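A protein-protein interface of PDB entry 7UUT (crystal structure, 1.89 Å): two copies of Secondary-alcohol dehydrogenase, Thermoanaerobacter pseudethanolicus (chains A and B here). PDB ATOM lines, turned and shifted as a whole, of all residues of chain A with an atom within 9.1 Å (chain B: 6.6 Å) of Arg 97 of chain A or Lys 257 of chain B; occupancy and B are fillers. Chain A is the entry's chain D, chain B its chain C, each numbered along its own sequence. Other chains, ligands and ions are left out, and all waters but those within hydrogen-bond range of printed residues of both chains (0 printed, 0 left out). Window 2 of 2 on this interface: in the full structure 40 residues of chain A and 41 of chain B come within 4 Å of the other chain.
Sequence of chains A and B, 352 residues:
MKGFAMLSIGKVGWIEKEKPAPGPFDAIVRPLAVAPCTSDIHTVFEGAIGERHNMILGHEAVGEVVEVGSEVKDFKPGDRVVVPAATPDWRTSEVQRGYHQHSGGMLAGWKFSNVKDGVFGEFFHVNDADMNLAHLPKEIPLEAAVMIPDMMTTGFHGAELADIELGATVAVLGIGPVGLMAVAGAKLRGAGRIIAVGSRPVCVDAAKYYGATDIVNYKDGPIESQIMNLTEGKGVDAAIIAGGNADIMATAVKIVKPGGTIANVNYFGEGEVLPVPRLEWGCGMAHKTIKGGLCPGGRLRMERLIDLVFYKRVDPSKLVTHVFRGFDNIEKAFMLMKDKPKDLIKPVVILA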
ATOM      1  N   THR A  92     -28.460   1.022  -8.553  1.00  0.00           N
ATOM      2  CA  THR A  92     -28.680   2.460  -8.507  1.00  0.00           C
ATOM      3  C   THR A  92     -29.794   2.819  -9.481  1.00  0.00           C
ATOM      4  O   THR A  92     -30.253   1.990 -10.273  1.00  0.00           O
ATOM      5  CB  THR A  92     -27.413   3.253  -8.858  1.00  0.00           C
ATOM      6  OG1 THR A  92     -26.989   2.912 -10.185  1.00  0.00           O
ATOM      7  CG2 THR A  92     -26.285   2.958  -7.871  1.00  0.00           C
ATOM      8  N   SER A  93     -30.208   4.088  -9.435  1.00  0.00           N
ATOM      9  CA  SER A  93     -31.252   4.558 -10.339  1.00  0.00           C
ATOM     10  C   SER A  93     -30.762   4.654 -11.778  1.00  0.00           C
ATOM     11  O   SER A  93     -31.550   4.468 -12.711  1.00  0.00           O
ATOM     12  CB  SER A  93     -31.776   5.914  -9.867  1.00  0.00           C
ATOM     13  OG  SER A  93     -30.743   6.885  -9.874  1.00  0.00           O
ATOM     14  N   GLU A  94     -29.472   4.942 -11.980  1.00  0.00           N
ATOM     15  CA  GLU A  94     -28.952   5.072 -13.337  1.00  0.00           C
ATOM     16  C   GLU A  94     -28.918   3.730 -14.056  1.00  0.00           C
ATOM     17  O   GLU A  94     -28.959   3.689 -15.293  1.00  0.00           O
ATOM     18  CB  GLU A  94     -27.556   5.699 -13.312  1.00  0.00           C
ATOM     19  CG  GLU A  94     -27.528   7.150 -12.834  1.00  0.00           C
ATOM     20  CD  GLU A  94     -27.367   7.278 -11.326  1.00  0.00           C
ATOM     21  OE1 GLU A  94     -27.322   6.238 -10.636  1.00  0.00           O
ATOM     22  OE2 GLU A  94     -27.278   8.422 -10.830  1.00  0.00           O
ATOM     23  N   VAL A  95     -28.840   2.629 -13.307  1.00  0.00           N
ATOM     24  CA  VAL A  95     -28.905   1.313 -13.931  1.00  0.00           C
ATOM     25  C   VAL A  95     -30.310   1.047 -14.460  1.00  0.00           C
ATOM     26  O   VAL A  95     -30.481   0.483 -15.548  1.00  0.00           O
ATOM     27  CB  VAL A  95     -28.445   0.231 -12.937  1.00  0.00           C
ATOM     28  CG1 VAL A  95     -28.755  -1.162 -13.469  1.00  0.00           C
ATOM     29  CG2 VAL A  95     -26.962   0.375 -12.669  1.00  0.00           C
ATOM     30  N   GLN A  96     -31.341   1.473 -13.718  1.00  0.00           N
ATOM     31  CA  GLN A  96     -32.709   1.314 -14.201  1.00  0.00           C
ATOM     32  C   GLN A  96     -32.999   2.185 -15.421  1.00  0.00           C
ATOM     33  O   GLN A  96     -33.929   1.876 -16.175  1.00  0.00           O
ATOM     34  CB  GLN A  96     -33.713   1.614 -13.079  1.00  0.00           C
ATOM     35  CG  GLN A  96     -33.529   0.751 -11.827  1.00  0.00           C
ATOM     36  CD  GLN A  96     -34.716   0.803 -10.865  1.00  0.00           C
ATOM     37  OE1 GLN A  96     -35.844   1.098 -11.260  1.00  0.00           O
ATOM     38  NE2 GLN A  96     -34.462   0.499  -9.597  1.00  0.00           N
ATOM     39  N   ARG A  97     -32.225   3.254 -15.642  1.00  0.00           N
ATOM     40  CA  ARG A  97     -32.344   4.054 -16.858  1.00  0.00           C
ATOM     41  C   ARG A  97     -31.547   3.483 -18.024  1.00  0.00           C
ATOM     42  O   ARG A  97     -31.700   3.964 -19.151  1.00  0.00           O
ATOM     43  CB  ARG A  97     -31.888   5.498 -16.610  1.00  0.00           C
ATOM     44  CG  ARG A  97     -32.885   6.353 -15.848  1.00  0.00           C
ATOM     45  CD  ARG A  97     -32.599   7.852 -15.967  1.00  0.00           C
ATOM     46  NE  ARG A  97     -31.301   8.232 -15.421  1.00  0.00           N
ATOM     47  CZ  ARG A  97     -30.285   8.685 -16.144  1.00  0.00           C
ATOM     48  NH1 ARG A  97     -30.384   8.843 -17.456  1.00  0.00           N
ATOM     49  NH2 ARG A  97     -29.140   8.989 -15.538  1.00  0.00           N
ATOM     50  N   GLY A  98     -30.698   2.490 -17.783  1.00  0.00           N
ATOM     51  CA  GLY A  98     -29.918   1.892 -18.844  1.00  0.00           C
ATOM     52  C   GLY A  98     -28.548   2.493 -19.050  1.00  0.00           C
ATOM     53  O   GLY A  98     -27.981   2.341 -20.140  1.00  0.00           O
ATOM     54  N   TYR A  99     -27.994   3.174 -18.044  1.00  0.00           N
ATOM     55  CA  TYR A  99     -26.678   3.799 -18.147  1.00  0.00           C
ATOM     56  C   TYR A  99     -25.855   3.389 -16.922  1.00  0.00           C
ATOM     57  O   TYR A  99     -25.625   4.181 -16.007  1.00  0.00           O
ATOM     58  CB  TYR A  99     -26.802   5.321 -18.268  1.00  0.00           C
ATOM     59  CG  TYR A  99     -27.379   5.765 -19.593  1.00  0.00           C
ATOM     60  CD1 TYR A  99     -26.573   5.884 -20.721  1.00  0.00           C
ATOM     61  CD2 TYR A  99     -28.734   6.054 -19.719  1.00  0.00           C
ATOM     62  CE1 TYR A  99     -27.101   6.281 -21.941  1.00  0.00           C
ATOM     63  CE2 TYR A  99     -29.271   6.454 -20.934  1.00  0.00           C
ATOM     64  CZ  TYR A  99     -28.452   6.564 -22.040  1.00  0.00           C
ATOM     65  OH  TYR A  99     -28.987   6.963 -23.246  1.00  0.00           O
ATOM     66  N   HIS A 100     -25.394   2.135 -16.922  1.00  0.00           N
ATOM     67  CA  HIS A 100     -24.596   1.646 -15.804  1.00  0.00           C
ATOM     68  C   HIS A 100     -23.257   2.364 -15.709  1.00  0.00           C
ATOM     69  O   HIS A 100     -22.683   2.454 -14.617  1.00  0.00           O
ATOM     70  CB  HIS A 100     -24.380   0.137 -15.923  1.00  0.00           C
ATOM     71  CG  HIS A 100     -23.583  -0.271 -17.124  1.00  0.00           C
ATOM     72  ND1 HIS A 100     -24.166  -0.763 -18.272  1.00  0.00           N
ATOM     73  CD2 HIS A 100     -22.248  -0.253 -17.358  1.00  0.00           C
ATOM     74  CE1 HIS A 100     -23.226  -1.036 -19.159  1.00  0.00           C
ATOM     75  NE2 HIS A 100     -22.053  -0.733 -18.631  1.00  0.00           N
ATOM     76  N   GLN A 101     -22.750   2.894 -16.830  1.00  0.00           N
ATOM     77  CA  GLN A 101     -21.496   3.640 -16.807  1.00  0.00           C
ATOM     78  C   GLN A 101     -21.549   4.823 -15.849  1.00  0.00           C
ATOM     79  O   GLN A 101     -20.501   5.274 -15.372  1.00  0.00           O
ATOM     80  CB  GLN A 101     -21.145   4.145 -18.211  1.00  0.00           C
ATOM     81  CG  GLN A 101     -20.978   3.057 -19.261  1.00  0.00           C
ATOM     82  CD  GLN A 101     -22.225   2.847 -20.103  1.00  0.00           C
ATOM     83  OE1 GLN A 101     -23.339   2.794 -19.587  1.00  0.00           O
ATOM     84  NE2 GLN A 101     -22.037   2.722 -21.411  1.00  0.00           N
ATOM     85  N   HIS A 102     -22.743   5.325 -15.553  1.00  0.00           N
ATOM     86  CA  HIS A 102     -22.926   6.470 -14.675  1.00  0.00           C
ATOM     87  C   HIS A 102     -23.696   6.080 -13.420  1.00  0.00           C
ATOM     88  O   HIS A 102     -24.390   6.902 -12.822  1.00  0.00           O
ATOM     89  CB  HIS A 102     -23.619   7.598 -15.435  1.00  0.00           C
ATOM     90  CG  HIS A 102     -23.002   7.861 -16.772  1.00  0.00           C
ATOM     91  ND1 HIS A 102     -21.769   8.462 -16.913  1.00  0.00           N
ATOM     92  CD2 HIS A 102     -23.416   7.549 -18.022  1.00  0.00           C
ATOM     93  CE1 HIS A 102     -21.464   8.535 -18.197  1.00  0.00           C
ATOM     94  NE2 HIS A 102     -22.446   7.989 -18.891  1.00  0.00           N
ATOM     95  N   SER A 103     -23.566   4.820 -13.013  1.00  0.00           N
ATOM     96  CA  SER A 103     -24.244   4.310 -11.827  1.00  0.00           C
ATOM     97  C   SER A 103     -23.676   4.985 -10.582  1.00  0.00           C
ATOM     98  O   SER A 103     -22.546   4.700 -10.170  1.00  0.00           O
ATOM     99  CB  SER A 103     -24.082   2.794 -11.756  1.00  0.00           C
ATOM    100  OG  SER A 103     -24.705   2.264 -10.601  1.00  0.00           O
ATOM    101  N   GLY A 104     -24.451   5.885  -9.986  1.00  0.00           N
ATOM    102  CA  GLY A 104     -24.010   6.612  -8.815  1.00  0.00           C
ATOM    103  C   GLY A 104     -23.357   7.949  -9.091  1.00  0.00           C
ATOM    104  O   GLY A 104     -22.780   8.537  -8.168  1.00  0.00           O
ATOM    105  N   GLY A 105     -23.429   8.446 -10.323  1.00  0.00           N
ATOM    106  CA  GLY A 105     -22.817   9.711 -10.682  1.00  0.00           C
ATOM    107  C   GLY A 105     -22.157   9.646 -12.044  1.00  0.00           C
ATOM    108  O   GLY A 105     -21.964   8.554 -12.584  1.00  0.00           O
ATOM    109  N   MET A 106     -21.795  10.798 -12.603  1.00  0.00           N
ATOM    110  CA  MET A 106     -21.182  10.825 -13.926  1.00  0.00           C
ATOM    111  C   MET A 106     -19.861  10.064 -13.923  1.00  0.00           C
ATOM    112  O   MET A 106     -18.973  10.338 -13.109  1.00  0.00           O
ATOM    113  CB  MET A 106     -20.960  12.268 -14.379  1.00  0.00           C
ATOM    114  CG  MET A 106     -20.641  12.416 -15.862  1.00  0.00           C
ATOM    115  SD  MET A 106     -20.630  14.141 -16.383  1.00  0.00           S
ATOM    116  CE  MET A 106     -22.121  14.746 -15.604  1.00  0.00           C
ATOM    117  N   THR B 169     -38.616  14.190 -16.410  1.00  0.00           N
ATOM    118  CA  THR B 169     -38.550  15.616 -16.120  1.00  0.00           C
ATOM    119  C   THR B 169     -37.876  16.326 -17.286  1.00  0.00           C
ATOM    120  O   THR B 169     -36.747  15.988 -17.659  1.00  0.00           O
ATOM    121  CB  THR B 169     -37.773  15.868 -14.827  1.00  0.00           C
ATOM    122  OG1 THR B 169     -38.472  15.283 -13.723  1.00  0.00           O
ATOM    123  CG2 THR B 169     -37.616  17.362 -14.584  1.00  0.00           C
ATOM    124  N   LYS B 234     -30.618  16.339  -9.101  1.00  0.00           N
ATOM    125  CA  LYS B 234     -30.704  15.270 -10.092  1.00  0.00           C
ATOM    126  C   LYS B 234     -30.534  15.785 -11.515  1.00  0.00           C
ATOM    127  O   LYS B 234     -30.053  15.050 -12.384  1.00  0.00           O
ATOM    128  CB  LYS B 234     -32.046  14.543  -9.978  1.00  0.00           C
ATOM    129  CG  LYS B 234     -32.243  13.743  -8.694  1.00  0.00           C
ATOM    130  CD  LYS B 234     -33.549  12.948  -8.737  1.00  0.00           C
ATOM    131  CE  LYS B 234     -34.724  13.729  -8.151  1.00  0.00           C
ATOM    132  NZ  LYS B 234     -35.171  14.863  -9.017  1.00  0.00           N
ATOM    133  N   GLY B 235     -30.919  17.024 -11.777  1.00  0.00           N
ATOM    134  CA  GLY B 235     -30.965  17.501 -13.136  1.00  0.00           C
ATOM    135  C   GLY B 235     -32.239  17.039 -13.817  1.00  0.00           C
ATOM    136  O   GLY B 235     -33.151  16.487 -13.196  1.00  0.00           O
ATOM    137  N   VAL B 236     -32.298  17.273 -15.121  1.00  0.00           N
ATOM    138  CA  VAL B 236     -33.463  16.907 -15.909  1.00  0.00           C
ATOM    139  C   VAL B 236     -33.082  15.768 -16.845  1.00  0.00           C
ATOM    140  O   VAL B 236     -31.913  15.571 -17.191  1.00  0.00           O
ATOM    141  CB  VAL B 236     -34.039  18.109 -16.692  1.00  0.00           C
ATOM    142  CG1 VAL B 236     -34.458  19.215 -15.735  1.00  0.00           C
ATOM    143  CG2 VAL B 236     -33.024  18.637 -17.704  1.00  0.00           C
ATOM    144  N   ASP B 237     -34.097  15.004 -17.256  1.00  0.00           N
ATOM    145  CA  ASP B 237     -33.867  13.902 -18.183  1.00  0.00           C
ATOM    146  C   ASP B 237     -33.614  14.410 -19.590  1.00  0.00           C
ATOM    147  O   ASP B 237     -32.900  13.767 -20.365  1.00  0.00           O
ATOM    148  CB  ASP B 237     -35.068  12.959 -18.183  1.00  0.00           C
ATOM    149  CG  ASP B 237     -35.314  12.345 -16.832  1.00  0.00           C
ATOM    150  OD1 ASP B 237     -34.484  11.518 -16.399  1.00  0.00           O
ATOM    151  OD2 ASP B 237     -36.323  12.713 -16.189  1.00  0.00           O
ATOM    152  N   ALA B 238     -34.190  15.555 -19.935  1.00  0.00           N
ATOM    153  CA  ALA B 238     -34.005  16.128 -21.254  1.00  0.00           C
ATOM    154  C   ALA B 238     -34.183  17.629 -21.162  1.00  0.00           C
ATOM    155  O   ALA B 238     -34.989  18.127 -20.373  1.00  0.00           O
ATOM    156  CB  ALA B 238     -34.989  15.541 -22.271  1.00  0.00           C
ATOM    157  N   ALA B 252     -27.647  23.951 -21.230  1.00  0.00           N
ATOM    158  CA  ALA B 252     -28.404  22.718 -21.410  1.00  0.00           C
ATOM    159  C   ALA B 252     -27.598  21.506 -20.967  1.00  0.00           C
ATOM    160  O   ALA B 252     -28.114  20.632 -20.260  1.00  0.00           O
ATOM    161  CB  ALA B 252     -28.833  22.575 -22.870  1.00  0.00           C
ATOM    162  N   VAL B 253     -26.318  21.450 -21.349  1.00  0.00           N
ATOM    163  CA  VAL B 253     -25.485  20.311 -20.976  1.00  0.00           C
ATOM    164  C   VAL B 253     -25.337  20.230 -19.463  1.00  0.00           C
ATOM    165  O   VAL B 253     -25.327  19.138 -18.882  1.00  0.00           O
ATOM    166  CB  VAL B 253     -24.116  20.399 -21.679  1.00  0.00           C
ATOM    167  CG1 VAL B 253     -23.179  19.310 -21.178  1.00  0.00           C
ATOM    168  CG2 VAL B 253     -24.291  20.290 -23.183  1.00  0.00           C
ATOM    169  N   LYS B 254     -25.255  21.382 -18.793  1.00  0.00           N
ATOM    170  CA  LYS B 254     -25.019  21.373 -17.354  1.00  0.00           C
ATOM    171  C   LYS B 254     -26.228  20.870 -16.571  1.00  0.00           C
ATOM    172  O   LYS B 254     -26.060  20.274 -15.500  1.00  0.00           O
ATOM    173  CB  LYS B 254     -24.617  22.769 -16.879  1.00  0.00           C
ATOM    174  CG  LYS B 254     -23.256  23.211 -17.396  1.00  0.00           C
ATOM    175  CD  LYS B 254     -22.947  24.651 -17.036  1.00  0.00           C
ATOM    176  CE  LYS B 254     -21.614  25.088 -17.627  1.00  0.00           C
ATOM    177  NZ  LYS B 254     -21.302  26.514 -17.322  1.00  0.00           N
ATOM    178  N   ILE B 255     -27.444  21.089 -17.076  1.00  0.00           N
ATOM    179  CA  ILE B 255     -28.632  20.709 -16.317  1.00  0.00           C
ATOM    180  C   ILE B 255     -29.151  19.314 -16.654  1.00  0.00           C
ATOM    181  O   ILE B 255     -29.924  18.748 -15.870  1.00  0.00           O
ATOM    182  CB  ILE B 255     -29.769  21.730 -16.505  1.00  0.00           C
ATOM    183  CG1 ILE B 255     -30.280  21.721 -17.947  1.00  0.00           C
ATOM    184  CG2 ILE B 255     -29.305  23.123 -16.120  1.00  0.00           C
ATOM    185  CD1 ILE B 255     -31.465  22.644 -18.171  1.00  0.00           C
ATOM    186  N   VAL B 256     -28.743  18.736 -17.781  1.00  0.00           N
ATOM    187  CA  VAL B 256     -29.190  17.397 -18.151  1.00  0.00           C
ATOM    188  C   VAL B 256     -28.363  16.366 -17.399  1.00  0.00           C
ATOM    189  O   VAL B 256     -27.141  16.506 -17.264  1.00  0.00           O
ATOM    190  CB  VAL B 256     -29.091  17.192 -19.673  1.00  0.00           C
ATOM    191  CG1 VAL B 256     -29.336  15.740 -20.037  1.00  0.00           C
ATOM    192  CG2 VAL B 256     -30.084  18.067 -20.379  1.00  0.00           C
ATOM    193  N   LYS B 257     -29.026  15.325 -16.895  1.00  0.00           N
ATOM    194  CA  LYS B 257     -28.325  14.275 -16.179  1.00  0.00           C
ATOM    195  C   LYS B 257     -27.558  13.383 -17.158  1.00  0.00           C
ATOM    196  O   LYS B 257     -27.843  13.374 -18.358  1.00  0.00           O
ATOM    197  CB  LYS B 257     -29.310  13.446 -15.360  1.00  0.00           C
ATOM    198  CG  LYS B 257     -30.313  12.670 -16.187  1.00  0.00           C
ATOM    199  CD  LYS B 257     -31.326  11.969 -15.297  1.00  0.00           C
ATOM    200  CE  LYS B 257     -32.084  12.981 -14.453  1.00  0.00           C
ATOM    201  NZ  LYS B 257     -33.246  12.380 -13.743  1.00  0.00           N
ATOM    202  N   PRO B 258     -26.558  12.646 -16.672  1.00  0.00           N
ATOM    203  CA  PRO B 258     -25.847  11.706 -17.548  1.00  0.00           C
ATOM    204  C   PRO B 258     -26.815  10.726 -18.193  1.00  0.00           C
ATOM    205  O   PRO B 258     -27.698  10.173 -17.535  1.00  0.00           O
ATOM    206  CB  PRO B 258     -24.880  10.998 -16.593  1.00  0.00           C
ATOM    207  CG  PRO B 258     -24.647  11.977 -15.507  1.00  0.00           C
ATOM    208  CD  PRO B 258     -25.948  12.710 -15.330  1.00  0.00           C
ATOM    209  N   GLY B 259     -26.650  10.522 -19.499  1.00  0.00           N
ATOM    210  CA  GLY B 259     -27.548   9.676 -20.251  1.00  0.00           C
ATOM    211  C   GLY B 259     -28.753  10.377 -20.836  1.00  0.00           C
ATOM    212  O   GLY B 259     -29.487   9.761 -21.620  1.00  0.00           O
ATOM    213  N   GLY B 260     -28.984  11.639 -20.481  1.00  0.00           N
ATOM    214  CA  GLY B 260     -30.109  12.392 -20.987  1.00  0.00           C
ATOM    215  C   GLY B 260     -29.837  12.940 -22.373  1.00  0.00           C
ATOM    216  O   GLY B 260     -28.834  12.631 -23.018  1.00  0.00           O
ATOM    217  N   THR B 261     -30.756  13.785 -22.835  1.00  0.00           N
ATOM    218  CA  THR B 261     -30.709  14.303 -24.194  1.00  0.00           C
ATOM    219  C   THR B 261     -30.868  15.815 -24.201  1.00  0.00           C
ATOM    220  O   THR B 261     -31.723  16.364 -23.502  1.00  0.00           O
ATOM    221  CB  THR B 261     -31.801  13.666 -25.063  1.00  0.00           C
ATOM    222  OG1 THR B 261     -31.672  12.241 -25.018  1.00  0.00           O
ATOM    223  CG2 THR B 261     -31.670  14.124 -26.510  1.00  0.00           C
ATOM    224  N   ALA B 286     -20.188  11.445 -21.015  1.00  0.00           N
ATOM    225  CA  ALA B 286     -21.322  11.509 -20.104  1.00  0.00           C
ATOM    226  C   ALA B 286     -22.609  10.965 -20.706  1.00  0.00           C
ATOM    227  O   ALA B 286     -23.653  11.032 -20.050  1.00  0.00           O
ATOM    228  CB  ALA B 286     -21.550  12.954 -19.647  1.00  0.00           C
ATOM    229  N   HIS B 287     -22.562  10.446 -21.935  1.00  0.00           N
ATOM    230  CA  HIS B 287     -23.755   9.973 -22.641  1.00  0.00           C
ATOM    231  C   HIS B 287     -24.830  11.048 -22.710  1.00  0.00           C
ATOM    232  O   HIS B 287     -26.027  10.753 -22.710  1.00  0.00           O
ATOM    233  CB  HIS B 287     -24.317   8.694 -22.011  1.00  0.00           C
ATOM    234  CG  HIS B 287     -23.549   7.459 -22.371  1.00  0.00           C
ATOM    235  ND1 HIS B 287     -22.526   6.963 -21.590  1.00  0.00           N
ATOM    236  CD2 HIS B 287     -23.640   6.632 -23.440  1.00  0.00           C
ATOM    237  CE1 HIS B 287     -22.034   5.873 -22.151  1.00  0.00           C
ATOM    238  NE2 HIS B 287     -22.686   5.655 -23.279  1.00  0.00           N
ATOM    239  N   LYS B 288     -24.420  12.310 -22.771  1.00  0.00           N
ATOM    240  CA  LYS B 288     -25.376  13.400 -22.940  1.00  0.00           C
ATOM    241  C   LYS B 288     -25.505  13.658 -24.435  1.00  0.00           C
ATOM    242  O   LYS B 288     -24.690  14.364 -25.034  1.00  0.00           O
ATOM    243  CB  LYS B 288     -24.938  14.636 -22.165  1.00  0.00           C
ATOM    244  CG  LYS B 288     -24.916  14.410 -20.655  1.00  0.00           C
ATOM    245  CD  LYS B 288     -24.647  15.697 -19.893  1.00  0.00           C
ATOM    246  CE  LYS B 288     -24.424  15.422 -18.418  1.00  0.00           C
ATOM    247  NZ  LYS B 288     -24.184  16.680 -17.660  1.00  0.00           N
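No position is printed for both chains.
Gln 96 of chain A touches none of the printed residues of chain B.
Arg 97 of chain A touches just these residues of chain B: Lys 257 (3.5 Å) and Pro 258 (2.7 Å).
Of the printed residues of chain B, His 102 of chain A touches Pro 258, Ala 286 and His 287.
Printed residues of chain B within 4 Å of Met 106 of chain A: Pro 258 (3.7 Å), Ala 286 (3.6 Å) and Lys 288 (3.5 Å).
Gly 235 of chain B touches none of the printed residues of chain A.
Of chain A, only Arg 97 (3.5 Å) comes within 4 Å of Lys 257 of chain B.
Of the printed residues of chain A, His 287 of chain B touches Tyr 99, Gln 101 and His 102.
The nearest residue of chain B that does not touch Arg 97 of chain A is Gly 259 of chain B (4.1 Å).
The nearest residue of chain A that does not touch Lys 257 of chain B is Met 106 of chain A (5.8 Å).
A ring nitrogen (NE2) of His 102 of chain A lies within hydrogen-bond range of a ring nitrogen (ND1) of His 287 of chain B, 2.9 Å away.
NE2 of His 102 of chain A lies within hydrogen-bond range of O of Ala 286 of chain B, 3.5 Å away.
OH of Tyr 99 of chain A lies within hydrogen-bond range of O of Gly 259 of chain B, at 3.3 Å.
The backbone carbonyl oxygen of Pro 258 of chain B sits at hydrogen-bond distance from the guanidinium group of Arg 97 of chain A.
Lys 257 of chain B touches Arg 97 of chain A (CD to CZ, 3.5 Å).
CB of His 287 of chain B touches CE1 of Tyr 99 of chain A (3.7 Å).
His 287 of chain B touches Gln 101 of chain A.
Pro 258 of chain B touches His 102 of chain A (CB to CG, 3.7 Å).
Met 106 of chain A touches Pro 258 of chain B.
Met 106 of chain A touches Ala 286 of chain B (SD to CB, 3.6 Å).
Lys 288 of chain B touches Met 106 of chain A.
The backbone carbonyl oxygen (O) of Ala 286 of chain B sits at hydrogen-bond distance from the backbone NH (N) of Gly 259 of chain B, 3.1 Å away.
O of Glu 94 of chain A sits at hydrogen-bond distance from N of Tyr 99 of chain A, at 3.0 Å.
O of Val 253 of chain B lies within hydrogen-bond range of NZ of Lys 288 of chain B (3.0 Å).
The side-chain amino group (NZ) of Lys 288 of chain B sits at hydrogen-bond distance from the backbone carbonyl oxygen (O) of Val 256 of chain B.
O of Val 236 of chain B is in hydrogen-bond range of N of Lys 257 of chain B, at 2.9 Å.
The backbone NH (N) of Gly 259 of chain B sits close to the backbone carbonyl oxygen (O) of His 287 of chain B (3.3 Å).
Of the 19 printed residues of chain B, 6 touch a printed residue of chain A.
Among the printed residues, no Asp or Glu carboxylate lies within 4 Å of a Lys or Arg side-chain nitrogen of the other chain.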
